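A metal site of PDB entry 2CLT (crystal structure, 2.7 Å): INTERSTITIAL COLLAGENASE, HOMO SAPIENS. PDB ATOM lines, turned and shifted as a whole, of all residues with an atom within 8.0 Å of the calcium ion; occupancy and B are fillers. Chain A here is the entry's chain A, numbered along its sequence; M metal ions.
The calcium ion is bound by O of Asp 186 (2.3 Å), O of Glu 230 (2.3 Å), O of Asp 279 (2.5 Å) and O of Asp 328 (2.7 Å).
Within 4 Å of the calcium ion: Asp 186, Glu 230, Asp 279 and Asp 328. Along chain A the residues within 4 Å of the calcium ion span positions 186 to 328.
ND1 of His 277 sits close to OD2 of Asp 279 (3.4 Å). N of Asp 279 sits at hydrogen-bond distance from O of Phe 293 (2.9 Å). The backbone NH (N) of Glu 230 lies within hydrogen-bond range of the backbone carbonyl oxygen (O) of Phe 244, at 3.0 Å. The backbone NH (N) of Asp 186 sits at hydrogen-bond distance from the backbone carbonyl oxygen (O) of Phe 198, at 3.0 Å. The side-chain carboxylate (OD1) of Asp 279 is in salt-bridge range of the side-chain amino group (NZ) of Lys 326. O of Phe 340 lies within hydrogen-bond range of N of Asp 328.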
ATOM      1  N   PHE A 185     -34.659  -2.110  -4.070  1.00  0.00           N
ATOM      2  CA  PHE A 185     -34.411  -3.072  -5.127  1.00  0.00           C
ATOM      3  C   PHE A 185     -33.124  -3.885  -5.021  1.00  0.00           C
ATOM      4  O   PHE A 185     -32.107  -3.369  -4.562  1.00  0.00           O
ATOM      5  CB  PHE A 185     -34.433  -2.358  -6.473  1.00  0.00           C
ATOM      6  CG  PHE A 185     -35.672  -1.552  -6.708  1.00  0.00           C
ATOM      7  CD1 PHE A 185     -36.917  -2.184  -6.779  1.00  0.00           C
ATOM      8  CD2 PHE A 185     -35.609  -0.176  -6.872  1.00  0.00           C
ATOM      9  CE1 PHE A 185     -38.070  -1.434  -7.008  1.00  0.00           C
ATOM     10  CE2 PHE A 185     -36.769   0.571  -7.095  1.00  0.00           C
ATOM     11  CZ  PHE A 185     -37.997  -0.063  -7.163  1.00  0.00           C
ATOM     12  N   ASP A 186     -33.190  -5.140  -5.479  1.00  0.00           N
ATOM     13  CA  ASP A 186     -32.020  -6.037  -5.490  1.00  0.00           C
ATOM     14  C   ASP A 186     -31.183  -5.691  -6.706  1.00  0.00           C
ATOM     15  O   ASP A 186     -29.959  -5.756  -6.653  1.00  0.00           O
ATOM     16  CB  ASP A 186     -32.421  -7.525  -5.603  1.00  0.00           C
ATOM     17  CG  ASP A 186     -33.216  -8.032  -4.409  1.00  0.00           C
ATOM     18  OD1 ASP A 186     -33.061  -7.463  -3.295  1.00  0.00           O
ATOM     19  OD2 ASP A 186     -33.979  -9.013  -4.567  1.00  0.00           O
ATOM     20  N   ALA A 187     -31.842  -5.334  -7.801  1.00  0.00           N
ATOM     21  CA  ALA A 187     -31.138  -4.982  -9.022  1.00  0.00           C
ATOM     22  C   ALA A 187     -32.096  -4.382 -10.038  1.00  0.00           C
ATOM     23  O   ALA A 187     -33.305  -4.571  -9.953  1.00  0.00           O
ATOM     24  CB  ALA A 187     -30.474  -6.208  -9.626  1.00  0.00           C
ATOM     25  N   ILE A 188     -31.549  -3.674 -11.017  1.00  0.00           N
ATOM     26  CA  ILE A 188     -32.366  -3.044 -12.049  1.00  0.00           C
ATOM     27  C   ILE A 188     -31.670  -3.059 -13.399  1.00  0.00           C
ATOM     28  O   ILE A 188     -30.451  -2.887 -13.483  1.00  0.00           O
ATOM     29  CB  ILE A 188     -32.669  -1.564 -11.701  1.00  0.00           C
ATOM     30  CG1 ILE A 188     -33.376  -1.453 -10.359  1.00  0.00           C
ATOM     31  CG2 ILE A 188     -33.535  -0.932 -12.803  1.00  0.00           C
ATOM     32  CD1 ILE A 188     -33.364  -0.049  -9.816  1.00  0.00           C
ATOM     33  N   PHE A 198     -36.031  -5.449 -10.092  1.00  0.00           N
ATOM     34  CA  PHE A 198     -36.079  -6.784  -9.512  1.00  0.00           C
ATOM     35  C   PHE A 198     -36.097  -6.732  -7.986  1.00  0.00           C
ATOM     36  O   PHE A 198     -35.391  -5.928  -7.372  1.00  0.00           O
ATOM     37  CB  PHE A 198     -34.886  -7.602  -9.991  1.00  0.00           C
ATOM     38  CG  PHE A 198     -34.906  -7.897 -11.451  1.00  0.00           C
ATOM     39  CD1 PHE A 198     -35.882  -8.716 -11.997  1.00  0.00           C
ATOM     40  CD2 PHE A 198     -33.969  -7.322 -12.310  1.00  0.00           C
ATOM     41  CE1 PHE A 198     -35.932  -8.964 -13.368  1.00  0.00           C
ATOM     42  CE2 PHE A 198     -34.012  -7.554 -13.680  1.00  0.00           C
ATOM     43  CZ  PHE A 198     -34.990  -8.386 -14.220  1.00  0.00           C
ATOM     44  N   LEU A 229     -31.643 -12.184  -7.345  1.00  0.00           N
ATOM     45  CA  LEU A 229     -30.663 -11.504  -8.177  1.00  0.00           C
ATOM     46  C   LEU A 229     -29.992 -10.386  -7.382  1.00  0.00           C
ATOM     47  O   LEU A 229     -30.587  -9.805  -6.482  1.00  0.00           O
ATOM     48  CB  LEU A 229     -31.346 -10.920  -9.404  1.00  0.00           C
ATOM     49  CG  LEU A 229     -32.142 -11.937 -10.224  1.00  0.00           C
ATOM     50  CD1 LEU A 229     -32.928 -11.216 -11.315  1.00  0.00           C
ATOM     51  CD2 LEU A 229     -31.205 -12.957 -10.803  1.00  0.00           C
ATOM     52  N   GLU A 230     -28.734 -10.087  -7.724  1.00  0.00           N
ATOM     53  CA  GLU A 230     -27.987  -9.050  -7.032  1.00  0.00           C
ATOM     54  C   GLU A 230     -27.631  -7.856  -7.918  1.00  0.00           C
ATOM     55  O   GLU A 230     -27.497  -6.733  -7.436  1.00  0.00           O
ATOM     56  CB  GLU A 230     -26.733  -9.658  -6.410  1.00  0.00           C
ATOM     57  CG  GLU A 230     -27.024 -10.563  -5.208  1.00  0.00           C
ATOM     58  CD  GLU A 230     -25.875 -11.536  -4.893  1.00  0.00           C
ATOM     59  OE1 GLU A 230     -25.852 -12.075  -3.775  1.00  0.00           O
ATOM     60  OE2 GLU A 230     -25.030 -11.765  -5.779  1.00  0.00           O
ATOM     61  N   ALA A 231     -27.463  -8.106  -9.215  1.00  0.00           N
ATOM     62  CA  ALA A 231     -27.148  -7.055 -10.178  1.00  0.00           C
ATOM     63  C   ALA A 231     -27.550  -7.496 -11.593  1.00  0.00           C
ATOM     64  O   ALA A 231     -27.835  -8.668 -11.804  1.00  0.00           O
ATOM     65  CB  ALA A 231     -25.676  -6.725 -10.140  1.00  0.00           C
ATOM     66  N   ALA A 232     -27.574  -6.557 -12.540  1.00  0.00           N
ATOM     67  CA  ALA A 232     -27.965  -6.897 -13.902  1.00  0.00           C
ATOM     68  C   ALA A 232     -27.877  -5.692 -14.834  1.00  0.00           C
ATOM     69  O   ALA A 232     -28.038  -4.550 -14.408  1.00  0.00           O
ATOM     70  CB  ALA A 232     -29.392  -7.450 -13.913  1.00  0.00           C
ATOM     71  N   PHE A 244     -26.402 -11.239 -12.333  1.00  0.00           N
ATOM     72  CA  PHE A 244     -25.361 -11.735 -11.440  1.00  0.00           C
ATOM     73  C   PHE A 244     -25.933 -12.203 -10.129  1.00  0.00           C
ATOM     74  O   PHE A 244     -26.824 -11.570  -9.578  1.00  0.00           O
ATOM     75  CB  PHE A 244     -24.323 -10.652 -11.150  1.00  0.00           C
ATOM     76  CG  PHE A 244     -23.555 -10.229 -12.355  1.00  0.00           C
ATOM     77  CD1 PHE A 244     -24.168  -9.476 -13.357  1.00  0.00           C
ATOM     78  CD2 PHE A 244     -22.235 -10.589 -12.516  1.00  0.00           C
ATOM     79  CE1 PHE A 244     -23.468  -9.108 -14.494  1.00  0.00           C
ATOM     80  CE2 PHE A 244     -21.531 -10.230 -13.651  1.00  0.00           C
ATOM     81  CZ  PHE A 244     -22.151  -9.480 -14.648  1.00  0.00           C
ATOM     82  N   HIS A 277     -19.330 -11.374  -4.250  1.00  0.00           N
ATOM     83  CA  HIS A 277     -20.454 -11.163  -5.168  1.00  0.00           C
ATOM     84  C   HIS A 277     -20.436  -9.770  -5.817  1.00  0.00           C
ATOM     85  O   HIS A 277     -19.384  -9.170  -5.988  1.00  0.00           O
ATOM     86  CB  HIS A 277     -21.776 -11.362  -4.421  1.00  0.00           C
ATOM     87  CG  HIS A 277     -21.924 -10.505  -3.207  1.00  0.00           C
ATOM     88  ND1 HIS A 277     -21.753  -9.140  -3.234  1.00  0.00           N
ATOM     89  CD2 HIS A 277     -22.262 -10.815  -1.927  1.00  0.00           C
ATOM     90  CE1 HIS A 277     -21.966  -8.649  -2.036  1.00  0.00           C
ATOM     91  NE2 HIS A 277     -22.282  -9.644  -1.223  1.00  0.00           N
ATOM     92  N   ILE A 278     -21.610  -9.282  -6.199  1.00  0.00           N
ATOM     93  CA  ILE A 278     -21.717  -7.965  -6.823  1.00  0.00           C
ATOM     94  C   ILE A 278     -22.990  -7.249  -6.362  1.00  0.00           C
ATOM     95  O   ILE A 278     -24.017  -7.886  -6.116  1.00  0.00           O
ATOM     96  CB  ILE A 278     -21.739  -8.074  -8.361  1.00  0.00           C
ATOM     97  CG1 ILE A 278     -20.411  -8.660  -8.850  1.00  0.00           C
ATOM     98  CG2 ILE A 278     -21.981  -6.704  -8.983  1.00  0.00           C
ATOM     99  CD1 ILE A 278     -20.293  -8.736 -10.354  1.00  0.00           C
ATOM    100  N   ASP A 279     -22.904  -5.929  -6.237  1.00  0.00           N
ATOM    101  CA  ASP A 279     -24.041  -5.151  -5.779  1.00  0.00           C
ATOM    102  C   ASP A 279     -24.894  -4.524  -6.887  1.00  0.00           C
ATOM    103  O   ASP A 279     -26.113  -4.454  -6.768  1.00  0.00           O
ATOM    104  CB  ASP A 279     -23.567  -4.058  -4.819  1.00  0.00           C
ATOM    105  CG  ASP A 279     -22.819  -4.620  -3.619  1.00  0.00           C
ATOM    106  OD1 ASP A 279     -22.523  -3.851  -2.670  1.00  0.00           O
ATOM    107  OD2 ASP A 279     -22.517  -5.835  -3.610  1.00  0.00           O
ATOM    108  N   ALA A 280     -24.257  -4.072  -7.968  1.00  0.00           N
ATOM    109  CA  ALA A 280     -25.008  -3.445  -9.054  1.00  0.00           C
ATOM    110  C   ALA A 280     -24.147  -3.213 -10.288  1.00  0.00           C
ATOM    111  O   ALA A 280     -22.929  -3.118 -10.186  1.00  0.00           O
ATOM    112  CB  ALA A 280     -25.577  -2.120  -8.579  1.00  0.00           C
ATOM    113  N   ALA A 281     -24.789  -3.104 -11.452  1.00  0.00           N
ATOM    114  CA  ALA A 281     -24.042  -2.900 -12.688  1.00  0.00           C
ATOM    115  C   ALA A 281     -24.803  -2.129 -13.754  1.00  0.00           C
ATOM    116  O   ALA A 281     -26.010  -2.254 -13.877  1.00  0.00           O
ATOM    117  CB  ALA A 281     -23.634  -4.250 -13.250  1.00  0.00           C
ATOM    118  N   PHE A 293     -20.260  -2.519  -9.419  1.00  0.00           N
ATOM    119  CA  PHE A 293     -20.116  -1.995  -8.063  1.00  0.00           C
ATOM    120  C   PHE A 293     -20.084  -3.079  -7.008  1.00  0.00           C
ATOM    121  O   PHE A 293     -20.977  -3.931  -6.934  1.00  0.00           O
ATOM    122  CB  PHE A 293     -21.259  -1.016  -7.763  1.00  0.00           C
ATOM    123  CG  PHE A 293     -21.271   0.184  -8.651  1.00  0.00           C
ATOM    124  CD1 PHE A 293     -20.679   1.378  -8.232  1.00  0.00           C
ATOM    125  CD2 PHE A 293     -21.837   0.134  -9.911  1.00  0.00           C
ATOM    126  CE1 PHE A 293     -20.669   2.492  -9.060  1.00  0.00           C
ATOM    127  CE2 PHE A 293     -21.828   1.235 -10.746  1.00  0.00           C
ATOM    128  CZ  PHE A 293     -21.238   2.418 -10.320  1.00  0.00           C
ATOM    129  N   LYS A 326     -22.211   2.977  -1.367  1.00  0.00           N
ATOM    130  CA  LYS A 326     -22.781   1.650  -1.604  1.00  0.00           C
ATOM    131  C   LYS A 326     -23.989   1.759  -2.513  1.00  0.00           C
ATOM    132  O   LYS A 326     -24.915   2.520  -2.260  1.00  0.00           O
ATOM    133  CB  LYS A 326     -23.185   0.953  -0.304  1.00  0.00           C
ATOM    134  CG  LYS A 326     -23.717  -0.449  -0.572  1.00  0.00           C
ATOM    135  CD  LYS A 326     -24.464  -1.010   0.615  1.00  0.00           C
ATOM    136  CE  LYS A 326     -25.133  -2.332   0.249  1.00  0.00           C
ATOM    137  NZ  LYS A 326     -24.159  -3.350  -0.254  1.00  0.00           N
ATOM    138  N   VAL A 327     -23.973   0.956  -3.574  1.00  0.00           N
ATOM    139  CA  VAL A 327     -25.056   0.957  -4.543  1.00  0.00           C
ATOM    140  C   VAL A 327     -25.905  -0.311  -4.420  1.00  0.00           C
ATOM    141  O   VAL A 327     -25.372  -1.414  -4.293  1.00  0.00           O
ATOM    142  CB  VAL A 327     -24.451   1.082  -5.957  1.00  0.00           C
ATOM    143  CG1 VAL A 327     -25.530   1.298  -6.982  1.00  0.00           C
ATOM    144  CG2 VAL A 327     -23.451   2.224  -5.972  1.00  0.00           C
ATOM    145  N   ASP A 328     -27.227  -0.136  -4.431  1.00  0.00           N
ATOM    146  CA  ASP A 328     -28.188  -1.239  -4.332  1.00  0.00           C
ATOM    147  C   ASP A 328     -28.525  -1.724  -5.744  1.00  0.00           C
ATOM    148  O   ASP A 328     -28.680  -2.919  -5.979  1.00  0.00           O
ATOM    149  CB  ASP A 328     -29.475  -0.763  -3.645  1.00  0.00           C
ATOM    150  CG  ASP A 328     -29.587  -1.258  -2.203  1.00  0.00           C
ATOM    151  OD1 ASP A 328     -28.537  -1.472  -1.553  1.00  0.00           O
ATOM    152  OD2 ASP A 328     -30.733  -1.416  -1.717  1.00  0.00           O
ATOM    153  N   ALA A 329     -28.628  -0.769  -6.659  1.00  0.00           N
ATOM    154  CA  ALA A 329     -28.932  -1.053  -8.053  1.00  0.00           C
ATOM    155  C   ALA A 329     -28.673   0.212  -8.817  1.00  0.00           C
ATOM    156  O   ALA A 329     -28.553   1.278  -8.236  1.00  0.00           O
ATOM    157  CB  ALA A 329     -30.396  -1.455  -8.204  1.00  0.00           C
ATOM    158  N   VAL A 330     -28.596   0.105 -10.141  1.00  0.00           N
ATOM    159  CA  VAL A 330     -28.356   1.249 -10.994  1.00  0.00           C
ATOM    160  C   VAL A 330     -28.643   0.890 -12.442  1.00  0.00           C
ATOM    161  O   VAL A 330     -28.429  -0.246 -12.867  1.00  0.00           O
ATOM    162  CB  VAL A 330     -26.890   1.743 -10.856  1.00  0.00           C
ATOM    163  CG1 VAL A 330     -25.936   0.640 -11.297  1.00  0.00           C
ATOM    164  CG2 VAL A 330     -26.671   2.968 -11.704  1.00  0.00           C
ATOM    165  N   PHE A 340     -29.513   3.618  -6.939  1.00  0.00           N
ATOM    166  CA  PHE A 340     -30.450   3.262  -5.895  1.00  0.00           C
ATOM    167  C   PHE A 340     -29.702   2.688  -4.701  1.00  0.00           C
ATOM    168  O   PHE A 340     -28.815   1.868  -4.852  1.00  0.00           O
ATOM    169  CB  PHE A 340     -31.471   2.229  -6.383  1.00  0.00           C
ATOM    170  CG  PHE A 340     -32.421   2.754  -7.397  1.00  0.00           C
ATOM    171  CD1 PHE A 340     -31.998   3.017  -8.701  1.00  0.00           C
ATOM    172  CD2 PHE A 340     -33.741   3.026  -7.058  1.00  0.00           C
ATOM    173  CE1 PHE A 340     -32.875   3.541  -9.649  1.00  0.00           C
ATOM    174  CE2 PHE A 340     -34.625   3.546  -7.999  1.00  0.00           C
ATOM    175  CZ  PHE A 340     -34.185   3.807  -9.300  1.00  0.00           C
HETATM  176 CA    CA M   1     -28.023  -5.468  -5.540  1.00  0.00          CA
